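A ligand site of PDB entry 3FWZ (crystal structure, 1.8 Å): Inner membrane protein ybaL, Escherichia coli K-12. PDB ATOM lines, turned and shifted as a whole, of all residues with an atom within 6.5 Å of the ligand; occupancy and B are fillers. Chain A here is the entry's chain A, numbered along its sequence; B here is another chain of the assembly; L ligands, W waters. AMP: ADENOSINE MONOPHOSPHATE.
N1 of the ligand is in hydrogen-bond range of N of Ala 58, 3.1 Å away.
The side-chain carboxylate (OE1) of Glu 37 is in hydrogen-bond range of an oxygen (O3') of the ligand (2.6 Å).
The backbone NH of Thr 38 sits at hydrogen-bond distance from a nitrogen (N3) of the ligand (3.4 Å).
N of Val 18 is in hydrogen-bond range of O1P of the ligand, at 3.0 Å.
The guanidinium group (NE) of Arg 17 is in salt-bridge range of an oxygen (O3P) of the ligand (2.9 Å).
An oxygen (O3P) of the ligand lies within hydrogen-bond range of the backbone NH of Arg 17 (2.8 Å).
O2P of the ligand lies within salt-bridge range of NH1 of Arg 104, at 2.9 Å.
The side-chain carboxylate (OE2) of Glu 84 is in hydrogen-bond range of a nitrogen (N6) of the ligand, at 2.9 Å.
An oxygen (O2') of the ligand sits at hydrogen-bond distance from the side-chain hydroxyl (OG1) of Thr 38 (3.2 Å).
N6 of the ligand is in hydrogen-bond range of OD1 of Asn 57 (2.9 Å).
Water W1 lies within hydrogen-bond range of O1P of the ligand (2.6 Å), OG1 of Thr 78 (2.8 Å), N of Gly 19 (2.8 Å) and N of Gly 16 (2.9 Å).
Water W6 bridges OE1 of Glu 84 and N7 of the ligand.
The backbone carbonyl oxygen (O) of Gly 14 sits at hydrogen-bond distance from the side-chain hydroxyl (OG1) of Thr 78.
OG of Ser 20 sits at hydrogen-bond distance from O of Gly 16 (2.7 Å).
The backbone carbonyl oxygen (O) of Glu 37 lies within hydrogen-bond range of the backbone NH (N) of Gly 56 (2.9 Å).
The side-chain amide oxygen (OD1) of Asn 57 sits at hydrogen-bond distance from the backbone NH (N) of Ala 59, at 2.9 Å.
The side-chain hydroxyl (OG) of Ser 39 is in hydrogen-bond range of the backbone NH (N) of Arg 42 (3.1 Å).
The side-chain carboxylate (OE1) of Glu 37 sits at hydrogen-bond distance from the backbone NH (N) of Tyr 15.
The backbone NH (N) of Ser 39 sits at hydrogen-bond distance from the side-chain carboxylate (OE2) of Glu 37, 3.0 Å away.
The guanidinium group of Arg 104 is in salt-bridge range of the side-chain carboxylate of Glu 126 of chain B, 3.1 Å away.
CG1 of Val 13 touches C2 of the ligand (3.7 Å).
CA of Gly 14 touches O4' of the ligand (3.5 Å).
CA of Gly 16 touches O5' of the ligand, 3.5 Å away.
O of Ile 36 touches C2 of the ligand, 3.99 Å away.
Arg 42 touches the ligand (NE to O3', 3.5 Å).
Gly 56 touches the ligand.
Thr 78 touches the ligand (O to O1P, 3.8 Å).
CG2 of Ile 79 touches N7 of the ligand (3.3 Å).
Hydrophobic or aromatic side chains within 4 Å of the ligand: Val 13, Val 18, Ala 58 and Ile 79.
Within 4 Å of the ligand: Val 13, Gly 14, Gly 16, Arg 17, Val 18, Ile 36, Glu 37, Thr 38, Arg 42, Gly 56, Asn 57, Ala 58, Thr 78, Ile 79, Glu 84 and Arg 104.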
ATOM      1  N   VAL A  13      25.617   6.340 -12.283  1.00  0.00           N
ATOM      2  CA  VAL A  13      24.294   6.042 -11.714  1.00  0.00           C
ATOM      3  C   VAL A  13      24.332   4.658 -11.074  1.00  0.00           C
ATOM      4  O   VAL A  13      24.521   3.646 -11.772  1.00  0.00           O
ATOM      5  CB  VAL A  13      23.183   6.074 -12.795  1.00  0.00           C
ATOM      6  CG1 VAL A  13      21.846   5.710 -12.179  1.00  0.00           C
ATOM      7  CG2 VAL A  13      23.111   7.462 -13.446  1.00  0.00           C
ATOM      8  N   GLY A  14      24.139   4.604  -9.754  1.00  0.00           N
ATOM      9  CA  GLY A  14      24.185   3.358  -9.011  1.00  0.00           C
ATOM     10  C   GLY A  14      25.530   3.111  -8.324  1.00  0.00           C
ATOM     11  O   GLY A  14      26.599   3.335  -8.881  1.00  0.00           O
ATOM     12  N   TYR A  15      25.480   2.678  -7.071  1.00  0.00           N
ATOM     13  CA  TYR A  15      26.702   2.362  -6.326  1.00  0.00           C
ATOM     14  C   TYR A  15      26.480   1.064  -5.560  1.00  0.00           C
ATOM     15  O   TYR A  15      26.745   0.978  -4.345  1.00  0.00           O
ATOM     16  CB  TYR A  15      27.070   3.508  -5.368  1.00  0.00           C
ATOM     17  CG  TYR A  15      28.575   3.722  -5.235  1.00  0.00           C
ATOM     18  CD1 TYR A  15      29.269   4.400  -6.231  1.00  0.00           C
ATOM     19  CD2 TYR A  15      29.274   3.193  -4.134  1.00  0.00           C
ATOM     20  CE1 TYR A  15      30.640   4.601  -6.131  1.00  0.00           C
ATOM     21  CE2 TYR A  15      30.658   3.382  -4.031  1.00  0.00           C
ATOM     22  CZ  TYR A  15      31.325   4.062  -5.043  1.00  0.00           C
ATOM     23  OH  TYR A  15      32.678   4.285  -4.954  1.00  0.00           O
ATOM     24  N   GLY A  16      25.963   0.059  -6.273  1.00  0.00           N
ATOM     25  CA  GLY A  16      25.730  -1.285  -5.732  1.00  0.00           C
ATOM     26  C   GLY A  16      26.930  -2.138  -6.088  1.00  0.00           C
ATOM     27  O   GLY A  16      28.063  -1.660  -6.106  1.00  0.00           O
ATOM     28  N   ARG A  17      26.663  -3.403  -6.434  1.00  0.00           N
ATOM     29  CA  ARG A  17      27.730  -4.350  -6.801  1.00  0.00           C
ATOM     30  C   ARG A  17      28.604  -3.819  -7.924  1.00  0.00           C
ATOM     31  O   ARG A  17      29.860  -3.941  -7.884  1.00  0.00           O
ATOM     32  CB  ARG A  17      27.116  -5.666  -7.253  1.00  0.00           C
ATOM     33  CG  ARG A  17      26.484  -6.462  -6.106  1.00  0.00           C
ATOM     34  CD  ARG A  17      25.593  -7.526  -6.684  1.00  0.00           C
ATOM     35  NE  ARG A  17      24.417  -6.940  -7.392  1.00  0.00           N
ATOM     36  CZ  ARG A  17      23.543  -7.652  -8.100  1.00  0.00           C
ATOM     37  NH1 ARG A  17      23.715  -8.974  -8.266  1.00  0.00           N
ATOM     38  NH2 ARG A  17      22.509  -7.036  -8.691  1.00  0.00           N
ATOM     39  N   VAL A  18      27.933  -3.298  -8.958  1.00  0.00           N
ATOM     40  CA  VAL A  18      28.663  -2.834 -10.159  1.00  0.00           C
ATOM     41  C   VAL A  18      29.252  -1.450  -9.930  1.00  0.00           C
ATOM     42  O   VAL A  18      30.452  -1.236 -10.103  1.00  0.00           O
ATOM     43  CB  VAL A  18      27.749  -2.801 -11.400  1.00  0.00           C
ATOM     44  CG1 VAL A  18      28.542  -2.318 -12.640  1.00  0.00           C
ATOM     45  CG2 VAL A  18      27.104  -4.188 -11.649  1.00  0.00           C
ATOM     46  N   GLY A  19      28.394  -0.509  -9.515  1.00  0.00           N
ATOM     47  CA  GLY A  19      28.825   0.899  -9.387  1.00  0.00           C
ATOM     48  C   GLY A  19      29.921   1.109  -8.351  1.00  0.00           C
ATOM     49  O   GLY A  19      30.820   1.961  -8.537  1.00  0.00           O
ATOM     50  N   SER A  20      29.887   0.347  -7.252  1.00  0.00           N
ATOM     51  CA  SER A  20      30.881   0.552  -6.196  1.00  0.00           C
ATOM     52  C   SER A  20      32.265   0.157  -6.712  1.00  0.00           C
ATOM     53  O   SER A  20      33.275   0.753  -6.352  1.00  0.00           O
ATOM     54  CB  SER A  20      30.537  -0.233  -4.910  1.00  0.00           C
ATOM     55  OG  SER A  20      30.540  -1.649  -5.147  1.00  0.00           O
ATOM     56  N   ILE A  36      24.976   9.288  -8.684  1.00  0.00           N
ATOM     57  CA  ILE A  36      23.558   9.416  -8.398  1.00  0.00           C
ATOM     58  C   ILE A  36      23.086   8.078  -7.829  1.00  0.00           C
ATOM     59  O   ILE A  36      23.337   7.026  -8.411  1.00  0.00           O
ATOM     60  CB  ILE A  36      22.743   9.747  -9.671  1.00  0.00           C
ATOM     61  CG1 ILE A  36      23.049  11.168 -10.126  1.00  0.00           C
ATOM     62  CG2 ILE A  36      21.237   9.662  -9.423  1.00  0.00           C
ATOM     63  CD1 ILE A  36      22.563  11.470 -11.566  1.00  0.00           C
ATOM     64  N   GLU A  37      22.416   8.139  -6.670  1.00  0.00           N
ATOM     65  CA  GLU A  37      21.807   6.945  -6.048  1.00  0.00           C
ATOM     66  C   GLU A  37      20.426   7.230  -5.501  1.00  0.00           C
ATOM     67  O   GLU A  37      20.198   8.289  -4.925  1.00  0.00           O
ATOM     68  CB  GLU A  37      22.687   6.403  -4.914  1.00  0.00           C
ATOM     69  CG  GLU A  37      23.447   5.145  -5.274  1.00  0.00           C
ATOM     70  CD  GLU A  37      22.557   3.909  -5.317  1.00  0.00           C
ATOM     71  OE1 GLU A  37      23.072   2.847  -5.688  1.00  0.00           O
ATOM     72  OE2 GLU A  37      21.359   3.974  -4.940  1.00  0.00           O
ATOM     73  N   THR A  38      19.512   6.274  -5.642  1.00  0.00           N
ATOM     74  CA  THR A  38      18.200   6.390  -4.938  1.00  0.00           C
ATOM     75  C   THR A  38      18.326   6.061  -3.450  1.00  0.00           C
ATOM     76  O   THR A  38      17.452   6.427  -2.643  1.00  0.00           O
ATOM     77  CB  THR A  38      17.148   5.448  -5.534  1.00  0.00           C
ATOM     78  OG1 THR A  38      17.723   4.140  -5.693  1.00  0.00           O
ATOM     79  CG2 THR A  38      16.644   5.951  -6.887  1.00  0.00           C
ATOM     80  N   SER A  39      19.402   5.371  -3.090  1.00  0.00           N
ATOM     81  CA  SER A  39      19.557   4.908  -1.709  1.00  0.00           C
ATOM     82  C   SER A  39      20.143   6.007  -0.841  1.00  0.00           C
ATOM     83  O   SER A  39      21.279   6.459  -1.056  1.00  0.00           O
ATOM     84  CB  SER A  39      20.432   3.645  -1.659  1.00  0.00           C
ATOM     85  OG  SER A  39      20.898   3.429  -0.328  1.00  0.00           O
ATOM     86  N   ARG A  42      23.401   4.778   0.828  1.00  0.00           N
ATOM     87  CA  ARG A  42      24.569   4.852  -0.049  1.00  0.00           C
ATOM     88  C   ARG A  42      25.053   6.287  -0.261  1.00  0.00           C
ATOM     89  O   ARG A  42      26.257   6.537  -0.217  1.00  0.00           O
ATOM     90  CB  ARG A  42      24.299   4.161  -1.366  1.00  0.00           C
ATOM     91  CG  ARG A  42      24.511   2.663  -1.235  1.00  0.00           C
ATOM     92  CD  ARG A  42      24.033   1.897  -2.450  1.00  0.00           C
ATOM     93  NE  ARG A  42      23.779   0.466  -2.167  1.00  0.00           N
ATOM     94  CZ  ARG A  42      24.403  -0.269  -1.232  1.00  0.00           C
ATOM     95  NH1 ARG A  42      25.351   0.246  -0.450  1.00  0.00           N
ATOM     96  NH2 ARG A  42      24.072  -1.528  -1.086  1.00  0.00           N
ATOM     97  N   GLY A  56      18.536  10.607  -5.455  1.00  0.00           N
ATOM     98  CA  GLY A  56      17.359  10.674  -6.324  1.00  0.00           C
ATOM     99  C   GLY A  56      17.455   9.692  -7.475  1.00  0.00           C
ATOM    100  O   GLY A  56      18.423   8.939  -7.598  1.00  0.00           O
ATOM    101  N   ASN A  57      16.439   9.709  -8.311  1.00  0.00           N
ATOM    102  CA  ASN A  57      16.333   8.748  -9.411  1.00  0.00           C
ATOM    103  C   ASN A  57      16.887   9.426 -10.654  1.00  0.00           C
ATOM    104  O   ASN A  57      16.495  10.550 -10.975  1.00  0.00           O
ATOM    105  CB  ASN A  57      14.855   8.384  -9.584  1.00  0.00           C
ATOM    106  CG  ASN A  57      14.644   7.209 -10.504  1.00  0.00           C
ATOM    107  OD1 ASN A  57      15.076   7.203 -11.647  1.00  0.00           O
ATOM    108  ND2 ASN A  57      13.930   6.203 -10.008  1.00  0.00           N
ATOM    109  N   ALA A  58      17.815   8.759 -11.322  1.00  0.00           N
ATOM    110  CA  ALA A  58      18.436   9.308 -12.548  1.00  0.00           C
ATOM    111  C   ALA A  58      17.459   9.539 -13.691  1.00  0.00           C
ATOM    112  O   ALA A  58      17.797  10.208 -14.654  1.00  0.00           O
ATOM    113  CB  ALA A  58      19.593   8.411 -13.025  1.00  0.00           C
ATOM    114  N   ALA A  59      16.261   8.943 -13.612  1.00  0.00           N
ATOM    115  CA  ALA A  59      15.187   9.220 -14.597  1.00  0.00           C
ATOM    116  C   ALA A  59      14.529  10.594 -14.381  1.00  0.00           C
ATOM    117  O   ALA A  59      13.752  11.053 -15.227  1.00  0.00           O
ATOM    118  CB  ALA A  59      14.140   8.120 -14.609  1.00  0.00           C
ATOM    119  N   THR A  78      24.726   1.866 -14.153  1.00  0.00           N
ATOM    120  CA  THR A  78      25.002   0.544 -13.589  1.00  0.00           C
ATOM    121  C   THR A  78      23.770  -0.107 -12.966  1.00  0.00           C
ATOM    122  O   THR A  78      23.888  -1.068 -12.207  1.00  0.00           O
ATOM    123  CB  THR A  78      26.171   0.581 -12.566  1.00  0.00           C
ATOM    124  OG1 THR A  78      25.728   1.183 -11.328  1.00  0.00           O
ATOM    125  CG2 THR A  78      27.369   1.331 -13.144  1.00  0.00           C
ATOM    126  N   ILE A  79      22.596   0.428 -13.278  1.00  0.00           N
ATOM    127  CA  ILE A  79      21.327  -0.117 -12.789  1.00  0.00           C
ATOM    128  C   ILE A  79      20.974  -1.420 -13.532  1.00  0.00           C
ATOM    129  O   ILE A  79      21.390  -1.618 -14.695  1.00  0.00           O
ATOM    130  CB  ILE A  79      20.195   0.927 -12.857  1.00  0.00           C
ATOM    131  CG1 ILE A  79      19.799   1.173 -14.334  1.00  0.00           C
ATOM    132  CG2 ILE A  79      20.695   2.201 -12.106  1.00  0.00           C
ATOM    133  CD1 ILE A  79      18.626   2.200 -14.576  1.00  0.00           C
ATOM    134  N   PRO A  80      20.246  -2.341 -12.867  1.00  0.00           N
ATOM    135  CA  PRO A  80      20.165  -3.675 -13.511  1.00  0.00           C
ATOM    136  C   PRO A  80      19.131  -3.787 -14.608  1.00  0.00           C
ATOM    137  O   PRO A  80      19.246  -4.668 -15.460  1.00  0.00           O
ATOM    138  CB  PRO A  80      19.798  -4.629 -12.354  1.00  0.00           C
ATOM    139  CG  PRO A  80      19.236  -3.759 -11.279  1.00  0.00           C
ATOM    140  CD  PRO A  80      19.879  -2.383 -11.443  1.00  0.00           C
ATOM    141  N   GLU A  84      14.707   0.341 -18.096  1.00  0.00           N
ATOM    142  CA  GLU A  84      14.840   1.577 -17.318  1.00  0.00           C
ATOM    143  C   GLU A  84      16.079   2.362 -17.760  1.00  0.00           C
ATOM    144  O   GLU A  84      16.032   3.600 -17.946  1.00  0.00           O
ATOM    145  CB  GLU A  84      14.929   1.243 -15.826  1.00  0.00           C
ATOM    146  CG  GLU A  84      14.917   2.497 -14.941  1.00  0.00           C
ATOM    147  CD  GLU A  84      15.046   2.188 -13.454  1.00  0.00           C
ATOM    148  OE1 GLU A  84      15.187   0.992 -13.085  1.00  0.00           O
ATOM    149  OE2 GLU A  84      15.037   3.172 -12.659  1.00  0.00           O
ATOM    150  N   ILE A  88      16.683   6.374 -19.667  1.00  0.00           N
ATOM    151  CA  ILE A  88      17.617   7.386 -19.166  1.00  0.00           C
ATOM    152  C   ILE A  88      18.572   7.764 -20.296  1.00  0.00           C
ATOM    153  O   ILE A  88      18.847   8.952 -20.541  1.00  0.00           O
ATOM    154  CB  ILE A  88      18.349   6.893 -17.922  1.00  0.00           C
ATOM    155  CG1 ILE A  88      17.368   6.786 -16.747  1.00  0.00           C
ATOM    156  CG2 ILE A  88      19.497   7.845 -17.546  1.00  0.00           C
ATOM    157  CD1 ILE A  88      17.832   5.878 -15.597  1.00  0.00           C
ATOM    158  N   ARG A 104      24.679  -0.967 -18.438  1.00  0.00           N
ATOM    159  CA  ARG A 104      24.594  -2.377 -18.099  1.00  0.00           C
ATOM    160  C   ARG A 104      23.306  -3.020 -18.658  1.00  0.00           C
ATOM    161  O   ARG A 104      22.245  -2.382 -18.748  1.00  0.00           O
ATOM    162  CB  ARG A 104      24.610  -2.486 -16.577  1.00  0.00           C
ATOM    163  CG  ARG A 104      24.184  -3.839 -15.981  1.00  0.00           C
ATOM    164  CD  ARG A 104      24.188  -3.680 -14.427  1.00  0.00           C
ATOM    165  NE  ARG A 104      23.780  -4.927 -13.739  1.00  0.00           N
ATOM    166  CZ  ARG A 104      23.505  -4.971 -12.442  1.00  0.00           C
ATOM    167  NH1 ARG A 104      23.540  -3.868 -11.718  1.00  0.00           N
ATOM    168  NH2 ARG A 104      23.156  -6.134 -11.864  1.00  0.00           N
ATOM    169  N   TYR B 107      26.682 -12.426  -6.403  1.00  0.00           N
ATOM    170  CA  TYR B 107      26.756 -11.730  -5.119  1.00  0.00           C
ATOM    171  C   TYR B 107      28.006 -12.173  -4.387  1.00  0.00           C
ATOM    172  O   TYR B 107      28.464 -13.315  -4.586  1.00  0.00           O
ATOM    173  CB  TYR B 107      25.538 -12.092  -4.264  1.00  0.00           C
ATOM    174  CG  TYR B 107      24.261 -11.456  -4.772  1.00  0.00           C
ATOM    175  CD1 TYR B 107      23.916 -10.155  -4.414  1.00  0.00           C
ATOM    176  CD2 TYR B 107      23.440 -12.167  -5.639  1.00  0.00           C
ATOM    177  CE1 TYR B 107      22.737  -9.571  -4.887  1.00  0.00           C
ATOM    178  CE2 TYR B 107      22.249 -11.573  -6.128  1.00  0.00           C
ATOM    179  CZ  TYR B 107      21.923 -10.313  -5.736  1.00  0.00           C
ATOM    180  OH  TYR B 107      20.774  -9.733  -6.221  1.00  0.00           O
ATOM    181  N   GLU B 126      28.498  -9.409 -11.953  1.00  0.00           N
ATOM    182  CA  GLU B 126      28.527  -7.967 -11.716  1.00  0.00           C
ATOM    183  C   GLU B 126      29.960  -7.438 -11.590  1.00  0.00           C
ATOM    184  O   GLU B 126      30.247  -6.272 -11.974  1.00  0.00           O
ATOM    185  CB  GLU B 126      27.626  -7.618 -10.525  1.00  0.00           C
ATOM    186  CG  GLU B 126      26.140  -7.573 -10.935  1.00  0.00           C
ATOM    187  CD  GLU B 126      25.567  -8.873 -11.499  1.00  0.00           C
ATOM    188  OE1 GLU B 126      25.951  -9.966 -11.052  1.00  0.00           O
ATOM    189  OE2 GLU B 126      24.648  -8.778 -12.332  1.00  0.00           O
HETATM  190  P   AMP L   1      23.722  -3.414  -8.241  1.00  0.00           P
HETATM  191  O1P AMP L   1      24.911  -2.914  -9.054  1.00  0.00           O
HETATM  192  O2P AMP L   1      22.631  -4.130  -9.004  1.00  0.00           O
HETATM  193  O3P AMP L   1      24.036  -4.098  -6.947  1.00  0.00           O
HETATM  194  O5' AMP L   1      22.935  -2.114  -7.638  1.00  0.00           O
HETATM  195  C5' AMP L   1      22.286  -1.166  -8.481  1.00  0.00           C
HETATM  196  C4' AMP L   1      22.195   0.134  -7.671  1.00  0.00           C
HETATM  197  O4' AMP L   1      21.526   1.095  -8.510  1.00  0.00           O
HETATM  198  C3' AMP L   1      21.339   0.027  -6.392  1.00  0.00           C
HETATM  199  O3' AMP L   1      22.124   0.450  -5.261  1.00  0.00           O
HETATM  200  C2' AMP L   1      20.161   0.974  -6.620  1.00  0.00           C
HETATM  201  O2' AMP L   1      19.840   1.775  -5.474  1.00  0.00           O
HETATM  202  C1' AMP L   1      20.625   1.888  -7.729  1.00  0.00           C
HETATM  203  N9  AMP L   1      19.589   2.364  -8.686  1.00  0.00           N
HETATM  204  C8  AMP L   1      18.731   1.571  -9.370  1.00  0.00           C
HETATM  205  N7  AMP L   1      17.954   2.325 -10.193  1.00  0.00           N
HETATM  206  C5  AMP L   1      18.333   3.615  -9.988  1.00  0.00           C
HETATM  207  C6  AMP L   1      17.931   4.913 -10.555  1.00  0.00           C
HETATM  208  N6  AMP L   1      16.945   4.931 -11.466  1.00  0.00           N
HETATM  209  N1  AMP L   1      18.577   6.022 -10.110  1.00  0.00           N
HETATM  210  C2  AMP L   1      19.574   5.972  -9.209  1.00  0.00           C
HETATM  211  N3  AMP L   1      19.995   4.811  -8.653  1.00  0.00           N
HETATM  212  C4  AMP L   1      19.410   3.630  -9.008  1.00  0.00           C
HETATM  213  O   HOH W   1      25.578  -0.449  -9.107  1.00  0.00           O
HETATM  214  O   HOH W   2      18.562  -1.705  -8.166  1.00  0.00           O
HETATM  215  O   HOH W   3      23.169  -3.877  -4.586  1.00  0.00           O
HETATM  216  O   HOH W   4      20.192  -4.046  -7.987  1.00  0.00           O
HETATM  217  O   HOH W   5      18.881   0.328  -3.514  1.00  0.00           O
HETATM  218  O   HOH W   6      15.556   0.944 -10.388  1.00  0.00           O
